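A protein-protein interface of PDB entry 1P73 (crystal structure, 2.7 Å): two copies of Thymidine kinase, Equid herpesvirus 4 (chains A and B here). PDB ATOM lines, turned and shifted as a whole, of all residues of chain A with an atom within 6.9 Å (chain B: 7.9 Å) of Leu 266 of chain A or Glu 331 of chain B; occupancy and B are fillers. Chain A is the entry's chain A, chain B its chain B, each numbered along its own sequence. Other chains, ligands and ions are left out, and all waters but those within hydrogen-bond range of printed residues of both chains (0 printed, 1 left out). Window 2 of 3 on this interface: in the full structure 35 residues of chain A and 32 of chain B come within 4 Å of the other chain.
Among the printed residues, merely in contact across the chains: Leu 266 of chain A with Glu 331 of chain B (3.5 Å), Trp 271 of chain A with Phe 328 of chain B (3.7 Å) and Trp 271 of chain A with Ala 324 of chain B (3.7 Å).
Leu 266 of chain A touches just one residue of chain B: Glu 331 (3.5 Å). Pro 41 of chain B touches none of the printed residues of chain A. Of the printed residues of chain A, Ala 324 of chain B touches Trp 271 (3.7 Å). Thr 327 of chain B touches none of the printed residues of chain A. Of the printed residues of chain A, Phe 328 of chain B touches Trp 271. Glu 331 of chain B touches just these residues of chain A: Leu 266 (3.5 Å), Glu 267 (3.0 Å) and Val 268 (3.1 Å). The nearest printed residue of chain B that does not touch Trp 271 of chain A is Thr 327 of chain B (4.4 Å).
No position is printed for both chains.
The backbone NH (N) of Glu 267 of chain A lies within hydrogen-bond range of the side-chain carboxylate (OE2) of Glu 331 of chain B (3.0 Å). The backbone NH of Val 268 of chain A is in hydrogen-bond range of the side-chain carboxylate of Glu 331 of chain B (3.1 Å).
Hydrophobic or aromatic side chains of chain A that line the printed part of chain B: Leu 266, Val 268 and Trp 271. Of the 20 printed residues of chain B, 3 touch a printed residue of chain A.
The guanidinium group (NH2) of Arg 214 of chain A lies within salt-bridge range of the side-chain carboxylate (OE1) of Glu 267 of chain A (3.3 Å). The backbone carbonyl oxygen (O) of Leu 258 of chain A is in hydrogen-bond range of the backbone NH (N) of Leu 266 of chain A, at 3.3 Å.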
ATOM      1  N   TRP A 213     -37.367  25.414  24.969  1.00  0.00           N
ATOM      2  CA  TRP A 213     -36.453  24.805  25.931  1.00  0.00           C
ATOM      3  C   TRP A 213     -35.819  25.781  26.934  1.00  0.00           C
ATOM      4  O   TRP A 213     -35.423  25.367  28.029  1.00  0.00           O
ATOM      5  CB  TRP A 213     -35.402  23.948  25.222  1.00  0.00           C
ATOM      6  CG  TRP A 213     -34.377  24.702  24.494  1.00  0.00           C
ATOM      7  CD1 TRP A 213     -34.350  24.963  23.166  1.00  0.00           C
ATOM      8  CD2 TRP A 213     -33.193  25.283  25.045  1.00  0.00           C
ATOM      9  NE1 TRP A 213     -33.229  25.691  22.846  1.00  0.00           N
ATOM     10  CE2 TRP A 213     -32.501  25.905  23.984  1.00  0.00           C
ATOM     11  CE3 TRP A 213     -32.648  25.356  26.342  1.00  0.00           C
ATOM     12  CZ2 TRP A 213     -31.295  26.588  24.171  1.00  0.00           C
ATOM     13  CZ3 TRP A 213     -31.460  26.031  26.528  1.00  0.00           C
ATOM     14  CH2 TRP A 213     -30.790  26.641  25.446  1.00  0.00           C
ATOM     15  N   ARG A 214     -35.732  27.061  26.568  1.00  0.00           N
ATOM     16  CA  ARG A 214     -35.182  28.095  27.459  1.00  0.00           C
ATOM     17  C   ARG A 214     -36.112  28.456  28.637  1.00  0.00           C
ATOM     18  O   ARG A 214     -35.630  28.849  29.697  1.00  0.00           O
ATOM     19  CB  ARG A 214     -34.780  29.357  26.675  1.00  0.00           C
ATOM     20  CG  ARG A 214     -33.453  29.235  25.901  1.00  0.00           C
ATOM     21  CD  ARG A 214     -33.088  30.465  25.048  1.00  0.00           C
ATOM     22  NE  ARG A 214     -31.853  30.273  24.271  1.00  0.00           N
ATOM     23  CZ  ARG A 214     -30.605  30.441  24.742  1.00  0.00           C
ATOM     24  NH1 ARG A 214     -30.378  30.798  26.003  1.00  0.00           N
ATOM     25  NH2 ARG A 214     -29.567  30.228  23.947  1.00  0.00           N
ATOM     26  N   GLN A 256     -22.815  18.912  33.183  1.00  0.00           N
ATOM     27  CA  GLN A 256     -21.577  19.674  33.303  1.00  0.00           C
ATOM     28  C   GLN A 256     -20.812  19.624  31.985  1.00  0.00           C
ATOM     29  O   GLN A 256     -20.205  20.616  31.580  1.00  0.00           O
ATOM     30  CB  GLN A 256     -20.714  19.172  34.473  1.00  0.00           C
ATOM     31  N   GLU A 257     -20.894  18.487  31.300  1.00  0.00           N
ATOM     32  CA  GLU A 257     -20.177  18.277  30.045  1.00  0.00           C
ATOM     33  C   GLU A 257     -20.481  19.306  28.946  1.00  0.00           C
ATOM     34  O   GLU A 257     -19.696  19.451  28.009  1.00  0.00           O
ATOM     35  CB  GLU A 257     -20.453  16.872  29.512  1.00  0.00           C
ATOM     36  CG  GLU A 257     -19.370  16.330  28.604  1.00  0.00           C
ATOM     37  CD  GLU A 257     -19.474  14.833  28.411  1.00  0.00           C
ATOM     38  OE1 GLU A 257     -20.253  14.193  29.165  1.00  0.00           O
ATOM     39  OE2 GLU A 257     -18.777  14.299  27.507  1.00  0.00           O
ATOM     40  N   LEU A 258     -21.608  20.007  29.061  1.00  0.00           N
ATOM     41  CA  LEU A 258     -22.058  20.929  28.022  1.00  0.00           C
ATOM     42  C   LEU A 258     -22.011  22.403  28.433  1.00  0.00           C
ATOM     43  O   LEU A 258     -22.343  23.290  27.635  1.00  0.00           O
ATOM     44  CB  LEU A 258     -23.460  20.540  27.529  1.00  0.00           C
ATOM     45  CG  LEU A 258     -23.598  19.160  26.866  1.00  0.00           C
ATOM     46  CD1 LEU A 258     -25.037  18.903  26.448  1.00  0.00           C
ATOM     47  CD2 LEU A 258     -22.648  18.976  25.683  1.00  0.00           C
ATOM     48  N   LEU A 259     -21.586  22.668  29.665  1.00  0.00           N
ATOM     49  CA  LEU A 259     -21.521  24.036  30.171  1.00  0.00           C
ATOM     50  C   LEU A 259     -20.092  24.555  30.228  1.00  0.00           C
ATOM     51  O   LEU A 259     -19.144  23.783  30.175  1.00  0.00           O
ATOM     52  CB  LEU A 259     -22.164  24.116  31.552  1.00  0.00           C
ATOM     53  CG  LEU A 259     -23.410  23.254  31.773  1.00  0.00           C
ATOM     54  CD1 LEU A 259     -23.676  23.066  33.272  1.00  0.00           C
ATOM     55  CD2 LEU A 259     -24.640  23.831  31.054  1.00  0.00           C
ATOM     56  N   ASP A 260     -19.941  25.869  30.326  1.00  0.00           N
ATOM     57  CA  ASP A 260     -18.630  26.475  30.531  1.00  0.00           C
ATOM     58  C   ASP A 260     -18.349  26.605  32.031  1.00  0.00           C
ATOM     59  O   ASP A 260     -19.115  26.090  32.848  1.00  0.00           O
ATOM     60  CB  ASP A 260     -18.513  27.823  29.784  1.00  0.00           C
ATOM     61  CG  ASP A 260     -19.406  28.930  30.366  1.00  0.00           C
ATOM     62  OD1 ASP A 260     -20.129  28.708  31.376  1.00  0.00           O
ATOM     63  OD2 ASP A 260     -19.438  30.080  29.854  1.00  0.00           O
ATOM     64  N   ASP A 261     -17.260  27.284  32.392  1.00  0.00           N
ATOM     65  CA  ASP A 261     -16.893  27.476  33.800  1.00  0.00           C
ATOM     66  C   ASP A 261     -18.054  28.052  34.628  1.00  0.00           C
ATOM     67  O   ASP A 261     -18.451  27.461  35.636  1.00  0.00           O
ATOM     68  CB  ASP A 261     -15.633  28.355  33.916  1.00  0.00           C
ATOM     69  N   GLY A 263     -21.103  27.955  34.350  1.00  0.00           N
ATOM     70  CA  GLY A 263     -22.320  27.146  34.326  1.00  0.00           C
ATOM     71  C   GLY A 263     -23.360  27.426  33.240  1.00  0.00           C
ATOM     72  O   GLY A 263     -24.454  26.868  33.277  1.00  0.00           O
ATOM     73  N   VAL A 264     -23.033  28.293  32.285  1.00  0.00           N
ATOM     74  CA  VAL A 264     -23.929  28.581  31.163  1.00  0.00           C
ATOM     75  C   VAL A 264     -23.626  27.634  29.999  1.00  0.00           C
ATOM     76  O   VAL A 264     -22.472  27.328  29.721  1.00  0.00           O
ATOM     77  CB  VAL A 264     -23.830  30.066  30.731  1.00  0.00           C
ATOM     78  CG1 VAL A 264     -24.647  30.344  29.476  1.00  0.00           C
ATOM     79  CG2 VAL A 264     -24.294  30.974  31.866  1.00  0.00           C
ATOM     80  N   ILE A 265     -24.668  27.141  29.340  1.00  0.00           N
ATOM     81  CA  ILE A 265     -24.492  26.248  28.204  1.00  0.00           C
ATOM     82  C   ILE A 265     -23.796  27.006  27.070  1.00  0.00           C
ATOM     83  O   ILE A 265     -24.148  28.159  26.773  1.00  0.00           O
ATOM     84  CB  ILE A 265     -25.857  25.662  27.751  1.00  0.00           C
ATOM     85  CG1 ILE A 265     -25.648  24.409  26.882  1.00  0.00           C
ATOM     86  CG2 ILE A 265     -26.750  26.744  27.065  1.00  0.00           C
ATOM     87  CD1 ILE A 265     -26.933  23.633  26.569  1.00  0.00           C
ATOM     88  N   LEU A 266     -22.792  26.367  26.466  1.00  0.00           N
ATOM     89  CA  LEU A 266     -22.120  26.904  25.292  1.00  0.00           C
ATOM     90  C   LEU A 266     -23.163  27.141  24.208  1.00  0.00           C
ATOM     91  O   LEU A 266     -24.135  26.383  24.120  1.00  0.00           O
ATOM     92  CB  LEU A 266     -21.054  25.920  24.799  1.00  0.00           C
ATOM     93  CG  LEU A 266     -19.650  25.904  25.428  1.00  0.00           C
ATOM     94  CD1 LEU A 266     -19.257  27.255  26.001  1.00  0.00           C
ATOM     95  CD2 LEU A 266     -19.517  24.833  26.506  1.00  0.00           C
ATOM     96  N   GLU A 267     -22.973  28.183  23.398  1.00  0.00           N
ATOM     97  CA  GLU A 267     -23.912  28.508  22.321  1.00  0.00           C
ATOM     98  C   GLU A 267     -24.066  27.389  21.268  1.00  0.00           C
ATOM     99  O   GLU A 267     -25.165  27.137  20.765  1.00  0.00           O
ATOM    100  CB  GLU A 267     -23.550  29.850  21.653  1.00  0.00           C
ATOM    101  CG  GLU A 267     -24.185  31.078  22.308  1.00  0.00           C
ATOM    102  CD  GLU A 267     -25.714  31.120  22.164  1.00  0.00           C
ATOM    103  OE1 GLU A 267     -26.438  30.599  23.063  1.00  0.00           O
ATOM    104  OE2 GLU A 267     -26.198  31.686  21.153  1.00  0.00           O
ATOM    105  N   VAL A 268     -22.975  26.708  20.947  1.00  0.00           N
ATOM    106  CA  VAL A 268     -23.029  25.670  19.937  1.00  0.00           C
ATOM    107  C   VAL A 268     -23.944  24.533  20.382  1.00  0.00           C
ATOM    108  O   VAL A 268     -24.571  23.882  19.546  1.00  0.00           O
ATOM    109  CB  VAL A 268     -21.624  25.137  19.597  1.00  0.00           C
ATOM    110  CG1 VAL A 268     -20.986  24.403  20.806  1.00  0.00           C
ATOM    111  CG2 VAL A 268     -21.671  24.253  18.355  1.00  0.00           C
ATOM    112  N   HIS A 269     -24.005  24.295  21.696  1.00  0.00           N
ATOM    113  CA  HIS A 269     -24.848  23.246  22.273  1.00  0.00           C
ATOM    114  C   HIS A 269     -26.288  23.704  22.339  1.00  0.00           C
ATOM    115  O   HIS A 269     -27.206  22.914  22.129  1.00  0.00           O
ATOM    116  CB  HIS A 269     -24.352  22.827  23.661  1.00  0.00           C
ATOM    117  CG  HIS A 269     -23.002  22.186  23.647  1.00  0.00           C
ATOM    118  ND1 HIS A 269     -22.608  21.302  22.664  1.00  0.00           N
ATOM    119  CD2 HIS A 269     -21.944  22.315  24.483  1.00  0.00           C
ATOM    120  CE1 HIS A 269     -21.366  20.910  22.897  1.00  0.00           C
ATOM    121  NE2 HIS A 269     -20.940  21.509  23.995  1.00  0.00           N
ATOM    122  N   ALA A 270     -26.469  24.984  22.641  1.00  0.00           N
ATOM    123  CA  ALA A 270     -27.763  25.633  22.542  1.00  0.00           C
ATOM    124  C   ALA A 270     -28.373  25.474  21.135  1.00  0.00           C
ATOM    125  O   ALA A 270     -29.554  25.124  21.001  1.00  0.00           O
ATOM    126  CB  ALA A 270     -27.641  27.106  22.921  1.00  0.00           C
ATOM    127  N   TRP A 271     -27.561  25.707  20.098  1.00  0.00           N
ATOM    128  CA  TRP A 271     -27.993  25.532  18.713  1.00  0.00           C
ATOM    129  C   TRP A 271     -28.521  24.119  18.469  1.00  0.00           C
ATOM    130  O   TRP A 271     -29.489  23.934  17.717  1.00  0.00           O
ATOM    131  CB  TRP A 271     -26.867  25.850  17.730  1.00  0.00           C
ATOM    132  CG  TRP A 271     -26.390  27.270  17.734  1.00  0.00           C
ATOM    133  CD1 TRP A 271     -26.984  28.356  18.338  1.00  0.00           C
ATOM    134  CD2 TRP A 271     -25.201  27.771  17.105  1.00  0.00           C
ATOM    135  NE1 TRP A 271     -26.234  29.489  18.120  1.00  0.00           N
ATOM    136  CE2 TRP A 271     -25.129  29.156  17.376  1.00  0.00           C
ATOM    137  CE3 TRP A 271     -24.177  27.186  16.343  1.00  0.00           C
ATOM    138  CZ2 TRP A 271     -24.087  29.955  16.901  1.00  0.00           C
ATOM    139  CZ3 TRP A 271     -23.141  27.981  15.883  1.00  0.00           C
ATOM    140  CH2 TRP A 271     -23.102  29.345  16.161  1.00  0.00           C
ATOM    141  N   PRO B  41     -14.615  29.135  10.874  1.00  0.00           N
ATOM    142  CA  PRO B  41     -13.489  28.199  10.785  1.00  0.00           C
ATOM    143  C   PRO B  41     -13.886  26.759  11.032  1.00  0.00           C
ATOM    144  O   PRO B  41     -15.028  26.489  11.385  1.00  0.00           O
ATOM    145  CB  PRO B  41     -12.555  28.676  11.896  1.00  0.00           C
ATOM    146  CG  PRO B  41     -13.459  29.305  12.891  1.00  0.00           C
ATOM    147  CD  PRO B  41     -14.579  29.928  12.116  1.00  0.00           C
ATOM    148  N   GLU B  42     -12.929  25.858  10.839  1.00  0.00           N
ATOM    149  CA  GLU B  42     -13.088  24.452  11.179  1.00  0.00           C
ATOM    150  C   GLU B  42     -13.364  24.274  12.667  1.00  0.00           C
ATOM    151  O   GLU B  42     -12.701  24.888  13.507  1.00  0.00           O
ATOM    152  CB  GLU B  42     -11.855  23.653  10.764  1.00  0.00           C
ATOM    153  CG  GLU B  42     -12.159  22.708   9.596  1.00  0.00           C
ATOM    154  CD  GLU B  42     -11.016  22.599   8.596  1.00  0.00           C
ATOM    155  OE1 GLU B  42      -9.860  22.900   8.971  1.00  0.00           O
ATOM    156  OE2 GLU B  42     -11.275  22.213   7.431  1.00  0.00           O
ATOM    157  N   PRO B  43     -14.355  23.438  12.985  1.00  0.00           N
ATOM    158  CA  PRO B  43     -14.800  23.250  14.373  1.00  0.00           C
ATOM    159  C   PRO B  43     -13.786  22.437  15.191  1.00  0.00           C
ATOM    160  O   PRO B  43     -14.086  21.327  15.639  1.00  0.00           O
ATOM    161  CB  PRO B  43     -16.118  22.496  14.210  1.00  0.00           C
ATOM    162  CG  PRO B  43     -15.987  21.785  12.903  1.00  0.00           C
ATOM    163  CD  PRO B  43     -15.111  22.601  12.033  1.00  0.00           C
ATOM    164  N   MET B  44     -12.597  23.008  15.388  1.00  0.00           N
ATOM    165  CA  MET B  44     -11.461  22.281  15.953  1.00  0.00           C
ATOM    166  C   MET B  44     -11.608  21.955  17.452  1.00  0.00           C
ATOM    167  O   MET B  44     -11.335  20.823  17.860  1.00  0.00           O
ATOM    168  CB  MET B  44     -10.150  23.014  15.656  1.00  0.00           C
ATOM    169  CG  MET B  44      -8.896  22.181  15.878  1.00  0.00           C
ATOM    170  SD  MET B  44      -8.577  20.945  14.585  1.00  0.00           S
ATOM    171  CE  MET B  44      -7.872  22.008  13.225  1.00  0.00           C
ATOM    172  N   ALA B  45     -12.048  22.920  18.263  1.00  0.00           N
ATOM    173  CA  ALA B  45     -12.326  22.657  19.677  1.00  0.00           C
ATOM    174  C   ALA B  45     -13.306  21.498  19.838  1.00  0.00           C
ATOM    175  O   ALA B  45     -13.077  20.581  20.614  1.00  0.00           O
ATOM    176  CB  ALA B  45     -12.862  23.880  20.348  1.00  0.00           C
ATOM    177  N   TYR B  46     -14.388  21.533  19.074  1.00  0.00           N
ATOM    178  CA  TYR B  46     -15.380  20.474  19.096  1.00  0.00           C
ATOM    179  C   TYR B  46     -14.751  19.082  18.960  1.00  0.00           C
ATOM    180  O   TYR B  46     -15.189  18.131  19.612  1.00  0.00           O
ATOM    181  CB  TYR B  46     -16.421  20.709  17.999  1.00  0.00           C
ATOM    182  CG  TYR B  46     -17.734  20.043  18.291  1.00  0.00           C
ATOM    183  CD1 TYR B  46     -18.765  20.744  18.909  1.00  0.00           C
ATOM    184  CD2 TYR B  46     -17.939  18.697  17.961  1.00  0.00           C
ATOM    185  CE1 TYR B  46     -19.973  20.123  19.195  1.00  0.00           C
ATOM    186  CE2 TYR B  46     -19.132  18.069  18.246  1.00  0.00           C
ATOM    187  CZ  TYR B  46     -20.148  18.785  18.865  1.00  0.00           C
ATOM    188  OH  TYR B  46     -21.338  18.159  19.141  1.00  0.00           O
ATOM    189  N   TRP B  47     -13.725  18.974  18.121  1.00  0.00           N
ATOM    190  CA  TRP B  47     -13.063  17.697  17.846  1.00  0.00           C
ATOM    191  C   TRP B  47     -12.047  17.277  18.912  1.00  0.00           C
ATOM    192  O   TRP B  47     -11.852  16.086  19.137  1.00  0.00           O
ATOM    193  CB  TRP B  47     -12.390  17.724  16.472  1.00  0.00           C
ATOM    194  CG  TRP B  47     -13.346  17.843  15.331  1.00  0.00           C
ATOM    195  CD1 TRP B  47     -14.659  17.470  15.316  1.00  0.00           C
ATOM    196  CD2 TRP B  47     -13.066  18.362  14.026  1.00  0.00           C
ATOM    197  NE1 TRP B  47     -15.214  17.737  14.087  1.00  0.00           N
ATOM    198  CE2 TRP B  47     -14.262  18.289  13.278  1.00  0.00           C
ATOM    199  CE3 TRP B  47     -11.926  18.884  13.411  1.00  0.00           C
ATOM    200  CZ2 TRP B  47     -14.352  18.712  11.957  1.00  0.00           C
ATOM    201  CZ3 TRP B  47     -12.016  19.310  12.090  1.00  0.00           C
ATOM    202  CH2 TRP B  47     -13.221  19.220  11.377  1.00  0.00           C
ATOM    203  N   THR B  49     -11.267  19.447  22.140  1.00  0.00           N
ATOM    204  CA  THR B  49     -11.236  20.180  23.395  1.00  0.00           C
ATOM    205  C   THR B  49     -12.556  20.220  24.180  1.00  0.00           C
ATOM    206  O   THR B  49     -12.535  20.422  25.397  1.00  0.00           O
ATOM    207  CB  THR B  49     -10.708  21.604  23.086  1.00  0.00           C
ATOM    208  OG1 THR B  49      -9.308  21.519  22.790  1.00  0.00           O
ATOM    209  CG2 THR B  49     -10.766  22.550  24.304  1.00  0.00           C
ATOM    210  N   LEU B  50     -13.696  20.027  23.514  1.00  0.00           N
ATOM    211  CA  LEU B  50     -14.992  20.127  24.207  1.00  0.00           C
ATOM    212  C   LEU B  50     -15.489  18.837  24.896  1.00  0.00           C
ATOM    213  O   LEU B  50     -16.387  18.890  25.748  1.00  0.00           O
ATOM    214  CB  LEU B  50     -16.070  20.712  23.295  1.00  0.00           C
ATOM    215  CG  LEU B  50     -15.993  22.221  23.033  1.00  0.00           C
ATOM    216  CD1 LEU B  50     -17.216  22.683  22.245  1.00  0.00           C
ATOM    217  CD2 LEU B  50     -15.824  23.067  24.313  1.00  0.00           C
ATOM    218  N   ALA B 324     -23.379  34.720  15.417  1.00  0.00           N
ATOM    219  CA  ALA B 324     -23.049  33.314  15.205  1.00  0.00           C
ATOM    220  C   ALA B 324     -21.559  33.147  14.968  1.00  0.00           C
ATOM    221  O   ALA B 324     -20.909  32.314  15.607  1.00  0.00           O
ATOM    222  CB  ALA B 324     -23.850  32.723  14.037  1.00  0.00           C
ATOM    223  N   ALA B 325     -21.026  33.960  14.057  1.00  0.00           N
ATOM    224  CA  ALA B 325     -19.634  33.854  13.670  1.00  0.00           C
ATOM    225  C   ALA B 325     -18.716  34.171  14.855  1.00  0.00           C
ATOM    226  O   ALA B 325     -17.733  33.454  15.082  1.00  0.00           O
ATOM    227  CB  ALA B 325     -19.339  34.749  12.475  1.00  0.00           C
ATOM    228  N   ARG B 326     -19.050  35.217  15.616  1.00  0.00           N
ATOM    229  CA  ARG B 326     -18.284  35.589  16.802  1.00  0.00           C
ATOM    230  C   ARG B 326     -18.322  34.445  17.806  1.00  0.00           C
ATOM    231  O   ARG B 326     -17.276  34.009  18.291  1.00  0.00           O
ATOM    232  CB  ARG B 326     -18.808  36.889  17.426  1.00  0.00           C
ATOM    233  N   THR B 327     -19.529  33.950  18.094  1.00  0.00           N
ATOM    234  CA  THR B 327     -19.712  32.794  18.965  1.00  0.00           C
ATOM    235  C   THR B 327     -18.880  31.611  18.465  1.00  0.00           C
ATOM    236  O   THR B 327     -18.146  31.012  19.243  1.00  0.00           O
ATOM    237  CB  THR B 327     -21.188  32.421  19.080  1.00  0.00           C
ATOM    238  N   PHE B 328     -18.954  31.308  17.169  1.00  0.00           N
ATOM    239  CA  PHE B 328     -18.275  30.136  16.626  1.00  0.00           C
ATOM    240  C   PHE B 328     -16.759  30.245  16.739  1.00  0.00           C
ATOM    241  O   PHE B 328     -16.117  29.331  17.239  1.00  0.00           O
ATOM    242  CB  PHE B 328     -18.694  29.879  15.176  1.00  0.00           C
ATOM    243  CG  PHE B 328     -18.625  28.428  14.767  1.00  0.00           C
ATOM    244  CD1 PHE B 328     -17.646  27.987  13.885  1.00  0.00           C
ATOM    245  CD2 PHE B 328     -19.543  27.506  15.254  1.00  0.00           C
ATOM    246  CE1 PHE B 328     -17.581  26.646  13.502  1.00  0.00           C
ATOM    247  CE2 PHE B 328     -19.479  26.167  14.875  1.00  0.00           C
ATOM    248  CZ  PHE B 328     -18.501  25.741  13.997  1.00  0.00           C
ATOM    249  N   ASN B 329     -16.201  31.369  16.290  1.00  0.00           N
ATOM    250  CA  ASN B 329     -14.759  31.619  16.356  1.00  0.00           C
ATOM    251  C   ASN B 329     -14.187  31.458  17.773  1.00  0.00           C
ATOM    252  O   ASN B 329     -13.147  30.805  17.958  1.00  0.00           O
ATOM    253  CB  ASN B 329     -14.418  33.012  15.802  1.00  0.00           C
ATOM    254  CG  ASN B 329     -14.236  33.026  14.281  1.00  0.00           C
ATOM    255  OD1 ASN B 329     -13.115  32.960  13.770  1.00  0.00           O
ATOM    256  ND2 ASN B 329     -15.345  33.137  13.555  1.00  0.00           N
ATOM    257  N   ALA B 330     -14.870  32.037  18.763  1.00  0.00           N
ATOM    258  CA  ALA B 330     -14.433  31.968  20.161  1.00  0.00           C
ATOM    259  C   ALA B 330     -14.589  30.577  20.780  1.00  0.00           C
ATOM    260  O   ALA B 330     -13.782  30.182  21.613  1.00  0.00           O
ATOM    261  CB  ALA B 330     -15.160  32.998  21.006  1.00  0.00           C
ATOM    262  N   GLU B 331     -15.612  29.834  20.371  1.00  0.00           N
ATOM    263  CA  GLU B 331     -15.886  28.527  20.959  1.00  0.00           C
ATOM    264  C   GLU B 331     -15.155  27.381  20.268  1.00  0.00           C
ATOM    265  O   GLU B 331     -15.195  26.250  20.755  1.00  0.00           O
ATOM    266  CB  GLU B 331     -17.397  28.255  21.005  1.00  0.00           C
ATOM    267  CG  GLU B 331     -18.137  29.167  21.972  1.00  0.00           C
ATOM    268  CD  GLU B 331     -19.576  28.760  22.244  1.00  0.00           C
ATOM    269  OE1 GLU B 331     -20.154  27.948  21.473  1.00  0.00           O
ATOM    270  OE2 GLU B 331     -20.138  29.278  23.242  1.00  0.00           O
ATOM    271  N   MET B 332     -14.488  27.661  19.149  1.00  0.00           N
ATOM    272  CA  MET B 332     -13.885  26.599  18.338  1.00  0.00           C
ATOM    273  C   MET B 332     -12.362  26.679  18.209  1.00  0.00           C
ATOM    274  O   MET B 332     -11.749  25.832  17.541  1.00  0.00           O
ATOM    275  CB  MET B 332     -14.527  26.535  16.945  1.00  0.00           C
ATOM    276  CG  MET B 332     -15.997  26.141  16.934  1.00  0.00           C
ATOM    277  SD  MET B 332     -16.316  24.437  17.456  1.00  0.00           S
ATOM    278  CE  MET B 332     -17.254  24.698  18.970  1.00  0.00           C
ATOM    279  N   GLY B 333     -11.760  27.682  18.850  1.00  0.00           N
ATOM    280  CA  GLY B 333     -10.340  27.964  18.689  1.00  0.00           C
ATOM    281  C   GLY B 333      -9.430  27.017  19.455  1.00  0.00           C
ATOM    282  O   GLY B 333      -9.605  26.813  20.664  1.00  0.00           O
ATOM    283  N   VAL B 334      -8.459  26.440  18.741  1.00  0.00           N
ATOM    284  CA  VAL B 334      -7.476  25.510  19.317  1.00  0.00           C
ATOM    285  C   VAL B 334      -8.145  24.412  20.155  1.00  0.00           C
ATOM    286  O   VAL B 334      -8.012  23.222  19.861  1.00  0.00           O
ATOM    287  CB  VAL B 334      -6.380  26.246  20.165  1.00  0.00           C
ATOM    288  CG1 VAL B 334      -5.187  25.320  20.460  1.00  0.00           C
ATOM    289  CG2 VAL B 334      -5.906  27.531  19.468  1.00  0.00           C
